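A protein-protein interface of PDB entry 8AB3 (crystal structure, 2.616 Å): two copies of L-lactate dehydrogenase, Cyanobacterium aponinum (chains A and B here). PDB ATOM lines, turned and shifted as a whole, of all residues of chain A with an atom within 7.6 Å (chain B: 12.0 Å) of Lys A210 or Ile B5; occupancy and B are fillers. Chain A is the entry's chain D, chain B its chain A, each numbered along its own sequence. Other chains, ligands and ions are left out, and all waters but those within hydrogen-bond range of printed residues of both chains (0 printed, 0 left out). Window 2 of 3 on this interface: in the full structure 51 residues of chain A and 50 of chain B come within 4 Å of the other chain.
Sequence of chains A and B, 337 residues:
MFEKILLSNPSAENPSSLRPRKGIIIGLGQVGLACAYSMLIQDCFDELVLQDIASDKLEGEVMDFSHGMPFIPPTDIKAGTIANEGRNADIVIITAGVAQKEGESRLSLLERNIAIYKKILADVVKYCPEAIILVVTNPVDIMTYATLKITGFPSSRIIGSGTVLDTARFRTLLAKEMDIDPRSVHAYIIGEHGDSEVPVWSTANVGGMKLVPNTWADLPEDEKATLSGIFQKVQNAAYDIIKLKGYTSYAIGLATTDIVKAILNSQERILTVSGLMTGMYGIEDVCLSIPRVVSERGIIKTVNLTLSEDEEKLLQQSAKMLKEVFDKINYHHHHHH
Met A178 touches Phe B2 (CG to CB, 3.5 Å).
Met A178 touches Leu B6.
Val A206 touches Ile B5 (CG2 to CG2, 3.7 Å).
CG2 of Ile B5 touches CG of Met A209 (3.9 Å).
Ile B5 touches Lys A210.
Leu A211 touches Phe B2 (CD1 to CE1, 3.9 Å).
Printed residues of chain B within 4 Å of Met A178: Phe B2 (3.5 Å) and Leu B6 (3.7 Å).
No residue of chain B comes within 4 Å of Ser A202.
Ala A204 touches none of the printed residues of chain B.
No residue of chain B comes within 4 Å of Asn A205.
Val A206 touches one residue of chain B.
No residue of chain B comes within 4 Å of Gly A207.
Of the printed residues of chain B, Met A209 touches Ile B5 (3.9 Å).
Of the printed residues of chain B, Lys A210 touches Ile B5.
Of chain B, only Phe B2 (3.9 Å) comes within 4 Å of Leu A211.
No residue of chain B comes within 4 Å of Val A212.
Of the printed residues of chain A, Phe B2 touches Met A178 (3.5 Å) and Leu A211 (3.9 Å).
No residue of chain A comes within 4 Å of Lys B4.
Ile B5 touches just these residues of chain A: Val A206 (3.7 Å), Met A209 (3.9 Å) and Lys A210 (3.9 Å).
Of the printed residues of chain A, Leu B6 touches Met A178.
The nearest residue of chain A that does not touch Ile B5 is Leu A211 (4.4 Å).
The nearest printed residue of chain A that does not touch Phe B2 is Trp A201 (6.0 Å).
O of Ala A204 is in hydrogen-bond range of N of Leu A211, 3.0 Å away.
No position is printed for both chains.
Of the 6 pairs that touch across the chains among the printed residues, none has its exchanged pair printed and touching as well.
Of the 9 printed residues of chain B, 3 touch a printed residue of chain A.
Hydrophobic or aromatic side chains of chain B within 4 Å of the printed part of chain A: Phe B2, Ile B5 and Leu B6.
Among the printed residues, 6 pairs touch across the chains.
Among the printed residues, no Asp or Glu carboxylate lies within 4 Å of a Lys or Arg side-chain nitrogen of the other chain.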
ATOM      1  N   MET A 178      28.230   1.481   1.514  1.00  0.00           N
ATOM      2  CA  MET A 178      29.186   1.651   2.611  1.00  0.00           C
ATOM      3  C   MET A 178      29.931   0.380   3.003  1.00  0.00           C
ATOM      4  O   MET A 178      30.869   0.457   3.788  1.00  0.00           O
ATOM      5  CB  MET A 178      28.481   2.249   3.838  1.00  0.00           C
ATOM      6  CG  MET A 178      28.144   3.703   3.646  1.00  0.00           C
ATOM      7  SD  MET A 178      27.032   4.449   4.864  1.00  0.00           S
ATOM      8  CE  MET A 178      25.624   3.402   4.689  1.00  0.00           C
ATOM      9  N   TRP A 201      14.543  10.900   4.397  1.00  0.00           N
ATOM     10  CA  TRP A 201      15.930  11.353   4.330  1.00  0.00           C
ATOM     11  C   TRP A 201      16.327  12.229   5.518  1.00  0.00           C
ATOM     12  O   TRP A 201      17.494  12.259   5.884  1.00  0.00           O
ATOM     13  CB  TRP A 201      16.197  12.124   3.033  1.00  0.00           C
ATOM     14  CG  TRP A 201      16.142  11.307   1.777  1.00  0.00           C
ATOM     15  CD1 TRP A 201      15.211  11.395   0.785  1.00  0.00           C
ATOM     16  CD2 TRP A 201      17.095  10.327   1.346  1.00  0.00           C
ATOM     17  NE1 TRP A 201      15.518  10.522  -0.230  1.00  0.00           N
ATOM     18  CE2 TRP A 201      16.666   9.853   0.088  1.00  0.00           C
ATOM     19  CE3 TRP A 201      18.267   9.797   1.905  1.00  0.00           C
ATOM     20  CZ2 TRP A 201      17.348   8.864  -0.607  1.00  0.00           C
ATOM     21  CZ3 TRP A 201      18.953   8.828   1.201  1.00  0.00           C
ATOM     22  CH2 TRP A 201      18.493   8.372  -0.042  1.00  0.00           C
ATOM     23  N   SER A 202      15.369  12.939   6.122  1.00  0.00           N
ATOM     24  CA  SER A 202      15.655  13.825   7.249  1.00  0.00           C
ATOM     25  C   SER A 202      16.235  13.128   8.484  1.00  0.00           C
ATOM     26  O   SER A 202      16.877  13.782   9.310  1.00  0.00           O
ATOM     27  CB  SER A 202      14.408  14.613   7.638  1.00  0.00           C
ATOM     28  OG  SER A 202      13.410  13.781   8.211  1.00  0.00           O
ATOM     29  N   THR A 203      15.988  11.821   8.630  1.00  0.00           N
ATOM     30  CA  THR A 203      16.480  11.083   9.782  1.00  0.00           C
ATOM     31  C   THR A 203      17.421   9.926   9.419  1.00  0.00           C
ATOM     32  O   THR A 203      17.937   9.289  10.334  1.00  0.00           O
ATOM     33  CB  THR A 203      15.309  10.598  10.661  1.00  0.00           C
ATOM     34  OG1 THR A 203      14.623   9.531  10.005  1.00  0.00           O
ATOM     35  CG2 THR A 203      14.336  11.697  11.018  1.00  0.00           C
ATOM     36  N   ALA A 204      17.635   9.634   8.115  1.00  0.00           N
ATOM     37  CA  ALA A 204      18.515   8.537   7.679  1.00  0.00           C
ATOM     38  C   ALA A 204      19.930   8.693   8.255  1.00  0.00           C
ATOM     39  O   ALA A 204      20.520   9.771   8.136  1.00  0.00           O
ATOM     40  CB  ALA A 204      18.571   8.482   6.162  1.00  0.00           C
ATOM     41  N   ASN A 205      20.466   7.634   8.889  1.00  0.00           N
ATOM     42  CA  ASN A 205      21.768   7.732   9.536  1.00  0.00           C
ATOM     43  C   ASN A 205      22.469   6.392   9.799  1.00  0.00           C
ATOM     44  O   ASN A 205      21.821   5.352   9.866  1.00  0.00           O
ATOM     45  CB  ASN A 205      21.597   8.471  10.883  1.00  0.00           C
ATOM     46  CG  ASN A 205      20.922   7.648  11.956  1.00  0.00           C
ATOM     47  OD1 ASN A 205      21.571   6.988  12.769  1.00  0.00           O
ATOM     48  ND2 ASN A 205      19.605   7.647  11.962  1.00  0.00           N
ATOM     49  N   VAL A 206      23.789   6.438  10.029  1.00  0.00           N
ATOM     50  CA  VAL A 206      24.566   5.281  10.448  1.00  0.00           C
ATOM     51  C   VAL A 206      25.365   5.713  11.684  1.00  0.00           C
ATOM     52  O   VAL A 206      26.075   6.724  11.643  1.00  0.00           O
ATOM     53  CB  VAL A 206      25.458   4.625   9.355  1.00  0.00           C
ATOM     54  CG1 VAL A 206      24.623   4.098   8.205  1.00  0.00           C
ATOM     55  CG2 VAL A 206      26.529   5.572   8.852  1.00  0.00           C
ATOM     56  N   GLY A 207      25.169   5.008  12.794  1.00  0.00           N
ATOM     57  CA  GLY A 207      25.845   5.316  14.051  1.00  0.00           C
ATOM     58  C   GLY A 207      25.593   6.719  14.572  1.00  0.00           C
ATOM     59  O   GLY A 207      26.472   7.323  15.192  1.00  0.00           O
ATOM     60  N   GLY A 208      24.403   7.250  14.308  1.00  0.00           N
ATOM     61  CA  GLY A 208      24.037   8.603  14.710  1.00  0.00           C
ATOM     62  C   GLY A 208      24.415   9.676  13.701  1.00  0.00           C
ATOM     63  O   GLY A 208      23.953  10.815  13.802  1.00  0.00           O
ATOM     64  N   MET A 209      25.256   9.334  12.722  1.00  0.00           N
ATOM     65  CA  MET A 209      25.709  10.271  11.709  1.00  0.00           C
ATOM     66  C   MET A 209      24.737  10.288  10.534  1.00  0.00           C
ATOM     67  O   MET A 209      24.623   9.293   9.820  1.00  0.00           O
ATOM     68  CB  MET A 209      27.123   9.886  11.244  1.00  0.00           C
ATOM     69  CG  MET A 209      27.675  10.783  10.174  1.00  0.00           C
ATOM     70  SD  MET A 209      27.850  12.499  10.711  1.00  0.00           S
ATOM     71  CE  MET A 209      28.596  13.197   9.282  1.00  0.00           C
ATOM     72  N   LYS A 210      24.050  11.420  10.324  1.00  0.00           N
ATOM     73  CA  LYS A 210      23.063  11.552   9.257  1.00  0.00           C
ATOM     74  C   LYS A 210      23.659  11.570   7.857  1.00  0.00           C
ATOM     75  O   LYS A 210      24.735  12.118   7.659  1.00  0.00           O
ATOM     76  CB  LYS A 210      22.194  12.797   9.479  1.00  0.00           C
ATOM     77  CG  LYS A 210      21.311  12.712  10.717  1.00  0.00           C
ATOM     78  CD  LYS A 210      20.224  13.771  10.730  1.00  0.00           C
ATOM     79  CE  LYS A 210      20.802  15.167  10.793  1.00  0.00           C
ATOM     80  NZ  LYS A 210      19.753  16.191  11.052  1.00  0.00           N
ATOM     81  N   LEU A 211      22.954  10.981   6.879  1.00  0.00           N
ATOM     82  CA  LEU A 211      23.417  10.986   5.493  1.00  0.00           C
ATOM     83  C   LEU A 211      23.168  12.348   4.830  1.00  0.00           C
ATOM     84  O   LEU A 211      23.948  12.765   3.976  1.00  0.00           O
ATOM     85  CB  LEU A 211      22.774   9.856   4.669  1.00  0.00           C
ATOM     86  CG  LEU A 211      22.890   8.433   5.224  1.00  0.00           C
ATOM     87  CD1 LEU A 211      22.328   7.438   4.241  1.00  0.00           C
ATOM     88  CD2 LEU A 211      24.333   8.060   5.536  1.00  0.00           C
ATOM     89  N   VAL A 212      22.073  13.032   5.217  1.00  0.00           N
ATOM     90  CA  VAL A 212      21.735  14.375   4.753  1.00  0.00           C
ATOM     91  C   VAL A 212      21.983  15.275   5.971  1.00  0.00           C
ATOM     92  O   VAL A 212      21.184  15.286   6.909  1.00  0.00           O
ATOM     93  CB  VAL A 212      20.276  14.464   4.261  1.00  0.00           C
ATOM     94  CG1 VAL A 212      19.952  15.875   3.774  1.00  0.00           C
ATOM     95  CG2 VAL A 212      20.008  13.435   3.166  1.00  0.00           C
ATOM     96  N   PRO A 213      23.146  15.947   6.014  1.00  0.00           N
ATOM     97  CA  PRO A 213      23.509  16.734   7.203  1.00  0.00           C
ATOM     98  C   PRO A 213      22.587  17.889   7.583  1.00  0.00           C
ATOM     99  O   PRO A 213      22.395  18.128   8.771  1.00  0.00           O
ATOM    100  CB  PRO A 213      24.911  17.245   6.875  1.00  0.00           C
ATOM    101  CG  PRO A 213      25.020  17.166   5.401  1.00  0.00           C
ATOM    102  CD  PRO A 213      24.214  15.977   4.998  1.00  0.00           C
ATOM    103  N   ASN A 214      22.049  18.625   6.602  1.00  0.00           N
ATOM    104  CA  ASN A 214      21.159  19.747   6.898  1.00  0.00           C
ATOM    105  C   ASN A 214      19.777  19.497   6.249  1.00  0.00           C
ATOM    106  O   ASN A 214      18.947  18.823   6.863  1.00  0.00           O
ATOM    107  CB  ASN A 214      21.815  21.080   6.494  1.00  0.00           C
ATOM    108  CG  ASN A 214      23.194  21.255   7.075  1.00  0.00           C
ATOM    109  OD1 ASN A 214      23.364  21.461   8.284  1.00  0.00           O
ATOM    110  ND2 ASN A 214      24.209  21.166   6.227  1.00  0.00           N
ATOM    111  N   THR A 215      19.534  19.995   5.017  1.00  0.00           N
ATOM    112  CA  THR A 215      18.293  19.752   4.282  1.00  0.00           C
ATOM    113  C   THR A 215      18.640  19.219   2.892  1.00  0.00           C
ATOM    114  O   THR A 215      19.752  19.441   2.406  1.00  0.00           O
ATOM    115  CB  THR A 215      17.416  21.017   4.192  1.00  0.00           C
ATOM    116  OG1 THR A 215      18.015  21.972   3.314  1.00  0.00           O
ATOM    117  CG2 THR A 215      17.128  21.642   5.550  1.00  0.00           C
ATOM    118  N   GLU A 223      25.433  14.709  -5.294  1.00  0.00           N
ATOM    119  CA  GLU A 223      25.013  13.914  -4.146  1.00  0.00           C
ATOM    120  C   GLU A 223      23.505  13.652  -4.212  1.00  0.00           C
ATOM    121  O   GLU A 223      23.055  12.550  -3.890  1.00  0.00           O
ATOM    122  CB  GLU A 223      25.382  14.624  -2.838  1.00  0.00           C
ATOM    123  CG  GLU A 223      26.873  14.869  -2.703  1.00  0.00           C
ATOM    124  CD  GLU A 223      27.320  15.236  -1.304  1.00  0.00           C
ATOM    125  OE1 GLU A 223      26.595  14.898  -0.341  1.00  0.00           O
ATOM    126  OE2 GLU A 223      28.392  15.869  -1.171  1.00  0.00           O
ATOM    127  N   MET B   1      30.259   6.326  -3.027  1.00  0.00           N
ATOM    128  CA  MET B   1      29.691   7.394  -2.207  1.00  0.00           C
ATOM    129  C   MET B   1      29.883   7.106  -0.692  1.00  0.00           C
ATOM    130  O   MET B   1      30.312   6.001  -0.329  1.00  0.00           O
ATOM    131  CB  MET B   1      28.203   7.571  -2.557  1.00  0.00           C
ATOM    132  N   PHE B   2      29.602   8.108   0.183  1.00  0.00           N
ATOM    133  CA  PHE B   2      29.677   7.948   1.630  1.00  0.00           C
ATOM    134  C   PHE B   2      31.095   7.874   2.197  1.00  0.00           C
ATOM    135  O   PHE B   2      31.293   7.381   3.311  1.00  0.00           O
ATOM    136  CB  PHE B   2      28.849   6.746   2.073  1.00  0.00           C
ATOM    137  CG  PHE B   2      27.395   6.836   1.685  1.00  0.00           C
ATOM    138  CD1 PHE B   2      26.624   7.913   2.075  1.00  0.00           C
ATOM    139  CD2 PHE B   2      26.797   5.837   0.938  1.00  0.00           C
ATOM    140  CE1 PHE B   2      25.283   7.990   1.723  1.00  0.00           C
ATOM    141  CE2 PHE B   2      25.457   5.913   0.592  1.00  0.00           C
ATOM    142  CZ  PHE B   2      24.708   6.988   0.987  1.00  0.00           C
ATOM    143  N   GLU B   3      32.072   8.413   1.470  1.00  0.00           N
ATOM    144  CA  GLU B   3      33.460   8.441   1.946  1.00  0.00           C
ATOM    145  C   GLU B   3      33.681   9.480   3.058  1.00  0.00           C
ATOM    146  O   GLU B   3      34.666   9.393   3.785  1.00  0.00           O
ATOM    147  CB  GLU B   3      34.435   8.693   0.787  1.00  0.00           C
ATOM    148  CG  GLU B   3      34.299   7.683  -0.337  1.00  0.00           C
ATOM    149  CD  GLU B   3      33.245   8.016  -1.374  1.00  0.00           C
ATOM    150  OE1 GLU B   3      32.685   9.137  -1.331  1.00  0.00           O
ATOM    151  OE2 GLU B   3      32.990   7.152  -2.242  1.00  0.00           O
ATOM    152  N   LYS B   4      32.786  10.472   3.171  1.00  0.00           N
ATOM    153  CA  LYS B   4      32.829  11.489   4.218  1.00  0.00           C
ATOM    154  C   LYS B   4      32.036  11.062   5.480  1.00  0.00           C
ATOM    155  O   LYS B   4      32.090  11.760   6.491  1.00  0.00           O
ATOM    156  CB  LYS B   4      32.286  12.813   3.676  1.00  0.00           C
ATOM    157  N   ILE B   5      31.301   9.933   5.425  1.00  0.00           N
ATOM    158  CA  ILE B   5      30.539   9.406   6.553  1.00  0.00           C
ATOM    159  C   ILE B   5      31.392   8.351   7.258  1.00  0.00           C
ATOM    160  O   ILE B   5      31.504   8.368   8.479  1.00  0.00           O
ATOM    161  CB  ILE B   5      29.187   8.807   6.079  1.00  0.00           C
ATOM    162  CG1 ILE B   5      28.421   9.771   5.133  1.00  0.00           C
ATOM    163  CG2 ILE B   5      28.332   8.349   7.262  1.00  0.00           C
ATOM    164  CD1 ILE B   5      27.924  11.040   5.758  1.00  0.00           C
ATOM    165  N   LEU B   6      32.000   7.440   6.486  1.00  0.00           N
ATOM    166  CA  LEU B   6      32.862   6.407   7.047  1.00  0.00           C
ATOM    167  C   LEU B   6      34.295   6.620   6.597  1.00  0.00           C
ATOM    168  O   LEU B   6      34.559   6.690   5.407  1.00  0.00           O
ATOM    169  CB  LEU B   6      32.383   5.002   6.662  1.00  0.00           C
ATOM    170  CG  LEU B   6      30.965   4.629   7.088  1.00  0.00           C
ATOM    171  CD1 LEU B   6      30.645   3.223   6.678  1.00  0.00           C
ATOM    172  CD2 LEU B   6      30.771   4.770   8.582  1.00  0.00           C
ATOM    173  N   LEU B   7      35.221   6.746   7.546  1.00  0.00           N
ATOM    174  CA  LEU B   7      36.625   6.975   7.231  1.00  0.00           C
ATOM    175  C   LEU B   7      37.365   5.647   7.219  1.00  0.00           C
ATOM    176  O   LEU B   7      37.368   4.933   8.218  1.00  0.00           O
ATOM    177  CB  LEU B   7      37.252   7.938   8.241  1.00  0.00           C
ATOM    178  CG  LEU B   7      36.482   9.236   8.514  1.00  0.00           C
ATOM    179  CD1 LEU B   7      37.226  10.089   9.512  1.00  0.00           C
ATOM    180  CD2 LEU B   7      36.244  10.039   7.240  1.00  0.00           C
ATOM    181  N   SER B   8      37.950   5.295   6.077  1.00  0.00           N
ATOM    182  CA  SER B   8      38.674   4.041   5.925  1.00  0.00           C
ATOM    183  C   SER B   8      39.926   4.010   6.804  1.00  0.00           C
ATOM    184  O   SER B   8      40.594   5.030   6.964  1.00  0.00           O
ATOM    185  CB  SER B   8      39.047   3.820   4.460  1.00  0.00           C
ATOM    186  N   ASN B   9      40.244   2.848   7.373  1.00  0.00           N
ATOM    187  CA  ASN B   9      41.422   2.705   8.222  1.00  0.00           C
ATOM    188  C   ASN B   9      42.542   2.013   7.436  1.00  0.00           C
ATOM    189  O   ASN B   9      42.419   0.831   7.110  1.00  0.00           O
ATOM    190  CB  ASN B   9      41.052   1.901   9.472  1.00  0.00           C
ATOM    191  CG  ASN B   9      42.153   1.704  10.477  1.00  0.00           C
ATOM    192  OD1 ASN B   9      43.145   2.459  10.528  1.00  0.00           O
ATOM    193  ND2 ASN B   9      41.983   0.684  11.312  1.00  0.00           N
